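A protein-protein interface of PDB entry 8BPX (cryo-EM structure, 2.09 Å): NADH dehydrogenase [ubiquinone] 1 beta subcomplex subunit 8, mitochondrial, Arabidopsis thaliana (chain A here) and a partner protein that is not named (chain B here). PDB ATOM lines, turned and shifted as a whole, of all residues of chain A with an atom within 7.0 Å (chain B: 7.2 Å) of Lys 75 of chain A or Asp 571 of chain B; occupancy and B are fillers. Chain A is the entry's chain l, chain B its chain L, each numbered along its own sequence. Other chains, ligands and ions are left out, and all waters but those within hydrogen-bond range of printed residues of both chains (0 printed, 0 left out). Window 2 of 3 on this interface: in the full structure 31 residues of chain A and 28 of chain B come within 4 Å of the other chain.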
ATOM      1  N   ALA A  70     -19.705 -25.383   3.224  1.00  0.00           N
ATOM      2  CA  ALA A  70     -19.778 -26.601   4.022  1.00  0.00           C
ATOM      3  C   ALA A  70     -18.444 -26.894   4.699  1.00  0.00           C
ATOM      4  O   ALA A  70     -18.182 -28.029   5.100  1.00  0.00           O
ATOM      5  CB  ALA A  70     -20.201 -27.777   3.154  1.00  0.00           C
ATOM      6  N   VAL A  73     -18.762 -22.980   7.928  1.00  0.00           N
ATOM      7  CA  VAL A  73     -19.879 -22.881   8.910  1.00  0.00           C
ATOM      8  C   VAL A  73     -20.162 -24.243   9.573  1.00  0.00           C
ATOM      9  O   VAL A  73     -19.977 -25.242   8.925  1.00  0.00           O
ATOM     10  CB  VAL A  73     -21.086 -22.197   8.229  1.00  0.00           C
ATOM     11  CG1 VAL A  73     -22.023 -21.525   9.217  1.00  0.00           C
ATOM     12  CG2 VAL A  73     -20.650 -21.229   7.147  1.00  0.00           C
ATOM     13  N   GLY A  74     -20.523 -24.278  10.858  1.00  0.00           N
ATOM     14  CA  GLY A  74     -20.861 -25.478  11.594  1.00  0.00           C
ATOM     15  C   GLY A  74     -22.189 -26.072  11.156  1.00  0.00           C
ATOM     16  O   GLY A  74     -22.946 -25.496  10.379  1.00  0.00           O
ATOM     17  N   LYS A  75     -22.472 -27.264  11.677  1.00  0.00           N
ATOM     18  CA  LYS A  75     -23.668 -27.995  11.271  1.00  0.00           C
ATOM     19  C   LYS A  75     -24.920 -27.379  11.893  1.00  0.00           C
ATOM     20  O   LYS A  75     -25.833 -26.932  11.185  1.00  0.00           O
ATOM     21  CB  LYS A  75     -23.507 -29.466  11.664  1.00  0.00           C
ATOM     22  CG  LYS A  75     -24.773 -30.240  11.980  1.00  0.00           C
ATOM     23  CD  LYS A  75     -24.508 -31.720  11.777  1.00  0.00           C
ATOM     24  CE  LYS A  75     -25.670 -32.589  12.198  1.00  0.00           C
ATOM     25  NZ  LYS A  75     -26.628 -32.798  11.082  1.00  0.00           N
ATOM     26  N   TYR A  76     -24.969 -27.328  13.224  1.00  0.00           N
ATOM     27  CA  TYR A  76     -26.131 -26.765  13.896  1.00  0.00           C
ATOM     28  C   TYR A  76     -26.196 -25.257  13.728  1.00  0.00           C
ATOM     29  O   TYR A  76     -27.287 -24.683  13.741  1.00  0.00           O
ATOM     30  CB  TYR A  76     -26.119 -27.150  15.373  1.00  0.00           C
ATOM     31  CG  TYR A  76     -26.384 -28.615  15.599  1.00  0.00           C
ATOM     32  CD1 TYR A  76     -27.682 -29.106  15.632  1.00  0.00           C
ATOM     33  CD2 TYR A  76     -25.339 -29.513  15.757  1.00  0.00           C
ATOM     34  CE1 TYR A  76     -27.930 -30.443  15.830  1.00  0.00           C
ATOM     35  CE2 TYR A  76     -25.580 -30.852  15.953  1.00  0.00           C
ATOM     36  CZ  TYR A  76     -26.876 -31.312  15.989  1.00  0.00           C
ATOM     37  OH  TYR A  76     -27.120 -32.649  16.188  1.00  0.00           O
ATOM     38  N   GLU A  77     -25.059 -24.611  13.611  1.00  0.00           N
ATOM     39  CA  GLU A  77     -25.035 -23.164  13.276  1.00  0.00           C
ATOM     40  C   GLU A  77     -25.659 -22.914  11.893  1.00  0.00           C
ATOM     41  O   GLU A  77     -26.376 -21.962  11.749  1.00  0.00           O
ATOM     42  CB  GLU A  77     -23.592 -22.708  13.259  1.00  0.00           C
ATOM     43  CG  GLU A  77     -23.493 -21.198  13.265  1.00  0.00           C
ATOM     44  CD  GLU A  77     -22.268 -20.638  12.587  1.00  0.00           C
ATOM     45  OE1 GLU A  77     -21.369 -21.433  12.257  1.00  0.00           O
ATOM     46  OE2 GLU A  77     -22.211 -19.409  12.403  1.00  0.00           O
ATOM     47  N   ALA A  78     -25.307 -23.713  10.909  1.00  0.00           N
ATOM     48  CA  ALA A  78     -25.942 -23.589   9.602  1.00  0.00           C
ATOM     49  C   ALA A  78     -27.438 -23.849   9.700  1.00  0.00           C
ATOM     50  O   ALA A  78     -28.239 -23.162   9.053  1.00  0.00           O
ATOM     51  CB  ALA A  78     -25.293 -24.542   8.602  1.00  0.00           C
ATOM     52  N   LEU A  79     -27.834 -24.835  10.509  1.00  0.00           N
ATOM     53  CA  LEU A  79     -29.259 -25.072  10.722  1.00  0.00           C
ATOM     54  C   LEU A  79     -29.932 -23.849  11.340  1.00  0.00           C
ATOM     55  O   LEU A  79     -31.040 -23.479  10.944  1.00  0.00           O
ATOM     56  CB  LEU A  79     -29.465 -26.306  11.597  1.00  0.00           C
ATOM     57  CG  LEU A  79     -30.880 -26.583  12.114  1.00  0.00           C
ATOM     58  CD1 LEU A  79     -31.810 -26.990  10.983  1.00  0.00           C
ATOM     59  CD2 LEU A  79     -30.850 -27.660  13.179  1.00  0.00           C
ATOM     60  N   ALA A  80     -29.272 -23.205  12.305  1.00  0.00           N
ATOM     61  CA  ALA A  80     -29.842 -22.020  12.942  1.00  0.00           C
ATOM     62  C   ALA A  80     -29.974 -20.860  11.961  1.00  0.00           C
ATOM     63  O   ALA A  80     -30.993 -20.159  11.950  1.00  0.00           O
ATOM     64  CB  ALA A  80     -28.994 -21.612  14.145  1.00  0.00           C
ATOM     65  N   PHE B 564     -27.270 -21.984   3.174  1.00  0.00           N
ATOM     66  CA  PHE B 564     -26.783 -23.239   3.830  1.00  0.00           C
ATOM     67  C   PHE B 564     -27.779 -24.370   3.570  1.00  0.00           C
ATOM     68  O   PHE B 564     -27.801 -25.324   4.317  1.00  0.00           O
ATOM     69  CB  PHE B 564     -26.407 -23.006   5.308  1.00  0.00           C
ATOM     70  CG  PHE B 564     -25.463 -21.898   5.660  1.00  0.00           C
ATOM     71  CD1 PHE B 564     -24.262 -21.743   4.994  1.00  0.00           C
ATOM     72  CD2 PHE B 564     -25.752 -21.056   6.718  1.00  0.00           C
ATOM     73  CE1 PHE B 564     -23.392 -20.728   5.347  1.00  0.00           C
ATOM     74  CE2 PHE B 564     -24.871 -20.057   7.084  1.00  0.00           C
ATOM     75  CZ  PHE B 564     -23.702 -19.889   6.391  1.00  0.00           C
ATOM     76  N   PHE B 565     -28.540 -24.271   2.492  1.00  0.00           N
ATOM     77  CA  PHE B 565     -29.598 -25.248   2.270  1.00  0.00           C
ATOM     78  C   PHE B 565     -29.018 -26.623   1.957  1.00  0.00           C
ATOM     79  O   PHE B 565     -29.435 -27.633   2.537  1.00  0.00           O
ATOM     80  CB  PHE B 565     -30.522 -24.770   1.151  1.00  0.00           C
ATOM     81  CG  PHE B 565     -31.931 -25.261   1.283  1.00  0.00           C
ATOM     82  CD1 PHE B 565     -32.260 -26.570   0.992  1.00  0.00           C
ATOM     83  CD2 PHE B 565     -32.924 -24.409   1.728  1.00  0.00           C
ATOM     84  CE1 PHE B 565     -33.564 -27.012   1.126  1.00  0.00           C
ATOM     85  CE2 PHE B 565     -34.223 -24.845   1.865  1.00  0.00           C
ATOM     86  CZ  PHE B 565     -34.544 -26.146   1.565  1.00  0.00           C
ATOM     87  N   ASP B 566     -28.041 -26.676   1.046  1.00  0.00           N
ATOM     88  CA  ASP B 566     -27.391 -27.942   0.726  1.00  0.00           C
ATOM     89  C   ASP B 566     -26.686 -28.525   1.939  1.00  0.00           C
ATOM     90  O   ASP B 566     -26.768 -29.732   2.190  1.00  0.00           O
ATOM     91  CB  ASP B 566     -26.395 -27.760  -0.421  1.00  0.00           C
ATOM     92  CG  ASP B 566     -27.067 -27.706  -1.771  1.00  0.00           C
ATOM     93  OD1 ASP B 566     -27.496 -28.770  -2.258  1.00  0.00           O
ATOM     94  OD2 ASP B 566     -27.160 -26.608  -2.352  1.00  0.00           O
ATOM     95  N   GLN B 567     -25.984 -27.682   2.698  1.00  0.00           N
ATOM     96  CA  GLN B 567     -25.305 -28.155   3.897  1.00  0.00           C
ATOM     97  C   GLN B 567     -26.286 -28.800   4.863  1.00  0.00           C
ATOM     98  O   GLN B 567     -26.061 -29.920   5.330  1.00  0.00           O
ATOM     99  CB  GLN B 567     -24.578 -27.005   4.583  1.00  0.00           C
ATOM    100  CG  GLN B 567     -24.160 -27.321   6.006  1.00  0.00           C
ATOM    101  CD  GLN B 567     -22.951 -26.532   6.452  1.00  0.00           C
ATOM    102  OE1 GLN B 567     -22.468 -25.659   5.739  1.00  0.00           O
ATOM    103  NE2 GLN B 567     -22.442 -26.856   7.630  1.00  0.00           N
ATOM    104  N   VAL B 568     -27.380 -28.104   5.178  1.00  0.00           N
ATOM    105  CA  VAL B 568     -28.335 -28.620   6.154  1.00  0.00           C
ATOM    106  C   VAL B 568     -28.971 -29.910   5.649  1.00  0.00           C
ATOM    107  O   VAL B 568     -29.081 -30.898   6.391  1.00  0.00           O
ATOM    108  CB  VAL B 568     -29.394 -27.553   6.487  1.00  0.00           C
ATOM    109  CG1 VAL B 568     -30.580 -28.180   7.195  1.00  0.00           C
ATOM    110  CG2 VAL B 568     -28.782 -26.464   7.353  1.00  0.00           C
ATOM    111  N   LEU B 569     -29.388 -29.930   4.380  1.00  0.00           N
ATOM    112  CA  LEU B 569     -30.005 -31.139   3.843  1.00  0.00           C
ATOM    113  C   LEU B 569     -29.043 -32.319   3.889  1.00  0.00           C
ATOM    114  O   LEU B 569     -29.406 -33.402   4.352  1.00  0.00           O
ATOM    115  CB  LEU B 569     -30.505 -30.909   2.419  1.00  0.00           C
ATOM    116  CG  LEU B 569     -31.988 -30.563   2.265  1.00  0.00           C
ATOM    117  CD1 LEU B 569     -32.453 -29.532   3.288  1.00  0.00           C
ATOM    118  CD2 LEU B 569     -32.293 -30.124   0.840  1.00  0.00           C
ATOM    119  N   ASN B 570     -27.802 -32.122   3.446  1.00  0.00           N
ATOM    120  CA  ASN B 570     -26.844 -33.220   3.457  1.00  0.00           C
ATOM    121  C   ASN B 570     -26.517 -33.667   4.878  1.00  0.00           C
ATOM    122  O   ASN B 570     -26.393 -34.866   5.144  1.00  0.00           O
ATOM    123  CB  ASN B 570     -25.573 -32.815   2.718  1.00  0.00           C
ATOM    124  CG  ASN B 570     -24.475 -33.834   2.864  1.00  0.00           C
ATOM    125  OD1 ASN B 570     -24.430 -34.821   2.134  1.00  0.00           O
ATOM    126  ND2 ASN B 570     -23.580 -33.608   3.818  1.00  0.00           N
ATOM    127  N   ASP B 571     -26.392 -32.716   5.806  1.00  0.00           N
ATOM    128  CA  ASP B 571     -25.991 -33.047   7.167  1.00  0.00           C
ATOM    129  C   ASP B 571     -27.080 -33.782   7.929  1.00  0.00           C
ATOM    130  O   ASP B 571     -26.774 -34.631   8.770  1.00  0.00           O
ATOM    131  CB  ASP B 571     -25.604 -31.781   7.930  1.00  0.00           C
ATOM    132  CG  ASP B 571     -24.247 -31.256   7.536  1.00  0.00           C
ATOM    133  OD1 ASP B 571     -23.707 -31.711   6.506  1.00  0.00           O
ATOM    134  OD2 ASP B 571     -23.714 -30.393   8.264  1.00  0.00           O
ATOM    135  N   PHE B 572     -28.347 -33.467   7.672  1.00  0.00           N
ATOM    136  CA  PHE B 572     -29.407 -34.023   8.494  1.00  0.00           C
ATOM    137  C   PHE B 572     -30.265 -35.068   7.796  1.00  0.00           C
ATOM    138  O   PHE B 572     -30.947 -35.831   8.484  1.00  0.00           O
ATOM    139  CB  PHE B 572     -30.311 -32.901   9.025  1.00  0.00           C
ATOM    140  CG  PHE B 572     -29.651 -32.026  10.052  1.00  0.00           C
ATOM    141  CD1 PHE B 572     -28.895 -30.930   9.665  1.00  0.00           C
ATOM    142  CD2 PHE B 572     -29.787 -32.292  11.406  1.00  0.00           C
ATOM    143  CE1 PHE B 572     -28.291 -30.118  10.606  1.00  0.00           C
ATOM    144  CE2 PHE B 572     -29.184 -31.485  12.350  1.00  0.00           C
ATOM    145  CZ  PHE B 572     -28.432 -30.395  11.949  1.00  0.00           C
ATOM    146  N   LEU B 573     -30.238 -35.146   6.467  1.00  0.00           N
ATOM    147  CA  LEU B 573     -31.124 -36.027   5.721  1.00  0.00           C
ATOM    148  C   LEU B 573     -30.353 -37.090   4.945  1.00  0.00           C
ATOM    149  O   LEU B 573     -30.562 -38.291   5.169  1.00  0.00           O
ATOM    150  CB  LEU B 573     -31.973 -35.137   4.798  1.00  0.00           C
ATOM    151  CG  LEU B 573     -32.950 -35.612   3.724  1.00  0.00           C
ATOM    152  CD1 LEU B 573     -32.257 -36.070   2.449  1.00  0.00           C
ATOM    153  CD2 LEU B 573     -33.853 -36.674   4.271  1.00  0.00           C
ATOM    154  N   VAL B 574     -29.444 -36.681   4.056  1.00  0.00           N
ATOM    155  CA  VAL B 574     -28.706 -37.637   3.236  1.00  0.00           C
ATOM    156  C   VAL B 574     -27.787 -38.486   4.102  1.00  0.00           C
ATOM    157  O   VAL B 574     -27.723 -39.711   3.953  1.00  0.00           O
ATOM    158  CB  VAL B 574     -27.918 -36.909   2.132  1.00  0.00           C
ATOM    159  CG1 VAL B 574     -27.510 -37.882   1.050  1.00  0.00           C
ATOM    160  CG2 VAL B 574     -28.745 -35.777   1.543  1.00  0.00           C
ATOM    161  N   ARG B 575     -27.060 -37.843   5.017  1.00  0.00           N
ATOM    162  CA  ARG B 575     -26.217 -38.581   5.946  1.00  0.00           C
ATOM    163  C   ARG B 575     -27.048 -39.495   6.838  1.00  0.00           C
ATOM    164  O   ARG B 575     -26.625 -40.609   7.149  1.00  0.00           O
ATOM    165  CB  ARG B 575     -25.370 -37.615   6.779  1.00  0.00           C
ATOM    166  CG  ARG B 575     -24.590 -38.295   7.895  1.00  0.00           C
ATOM    167  CD  ARG B 575     -23.179 -37.748   8.140  1.00  0.00           C
ATOM    168  NE  ARG B 575     -22.879 -36.458   7.528  1.00  0.00           N
ATOM    169  CZ  ARG B 575     -23.328 -35.289   7.966  1.00  0.00           C
ATOM    170  NH1 ARG B 575     -24.138 -35.205   9.009  1.00  0.00           N
ATOM    171  NH2 ARG B 575     -22.943 -34.177   7.349  1.00  0.00           N
ATOM    172  N   SER B 576     -28.240 -39.051   7.243  1.00  0.00           N
ATOM    173  CA  SER B 576     -29.103 -39.896   8.060  1.00  0.00           C
ATOM    174  C   SER B 576     -29.463 -41.187   7.336  1.00  0.00           C
ATOM    175  O   SER B 576     -29.304 -42.284   7.882  1.00  0.00           O
ATOM    176  CB  SER B 576     -30.368 -39.134   8.457  1.00  0.00           C
ATOM    177  OG  SER B 576     -30.199 -38.470   9.690  1.00  0.00           O
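Gln 567 of chain B touches Ala 70 of chain A (OE1 to CA, 3.3 Å).
CG2 of Val 73 of chain A touches CE1 of Phe 564 of chain B, 3.3 Å away.
NZ of Lys 75 of chain A touches CZ of Phe 572 of chain B (3.1 Å).
Tyr 76 of chain A touches Phe 572 of chain B.
Ala 78 of chain A touches Phe 564 of chain B (CB to CB, 3.8 Å).
Gln 567 of chain B touches Ala 78 of chain A.
CG2 of Val 568 of chain B touches O of Ala 78 of chain A (3.8 Å).
N of Leu 79 of chain A touches CG2 of Val 568 of chain B, at 3.7 Å.
CZ of Phe 572 of chain B touches CD2 of Leu 79 of chain A (3.9 Å).
Of the 9 printed residues of chain A, 7 touch a printed residue of chain B.
Among the printed residues, no Asp or Glu carboxylate lies within 4 Å of a Lys or Arg side-chain nitrogen of the other chain.
Printed residues of chain B within 4 Å of Gly 74 of chain A: Gln 567.
Printed residues of chain B within 4 Å of Tyr 76 of chain A: Phe 572 (3.8 Å).
Printed residues of chain B within 4 Å of Leu 79 of chain A: Val 568 (3.7 Å) and Phe 572 (3.9 Å).
Printed residues of chain A within 4 Å of Phe 564 of chain B: Val 73 and Ala 78.
Asp 571 of chain B touches one residue of chain A.
Printed residues of chain A within 4 Å of Phe 572 of chain B: Lys 75, Tyr 76 and Leu 79.
The nearest residue of chain A that does not touch Asp 571 of chain B is Gly 74 of chain A (5.4 Å).
The nearest printed residue of chain B that does not touch Val 73 of chain A is Asp 571 of chain B (6.4 Å).
The side-chain carboxylate (OD1) of Asp 571 of chain B lies within hydrogen-bond range of the side-chain amide nitrogen (ND2) of Asn 570 of chain B, 3.3 Å away.
The guanidinium group of Arg 575 of chain B is in salt-bridge range of the side-chain carboxylate of Asp 571 of chain B (2.7 Å).
O of Phe 572 of chain B sits at hydrogen-bond distance from OG of Ser 576 of chain B (3.0 Å).
N of Gly 74 of chain A sits at hydrogen-bond distance from OE1 of Glu 77 of chain A, at 3.3 Å.
The side-chain amide nitrogen of Gln 567 of chain B is in hydrogen-bond range of the backbone carbonyl oxygen of Val 73 of chain A (3.2 Å).
NE2 of Gln 567 of chain B lies within hydrogen-bond range of O of Gly 74 of chain A (3.1 Å).
The backbone carbonyl oxygen (O) of Asp 571 of chain B is in hydrogen-bond range of the side-chain amino group (NZ) of Lys 75 of chain A.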
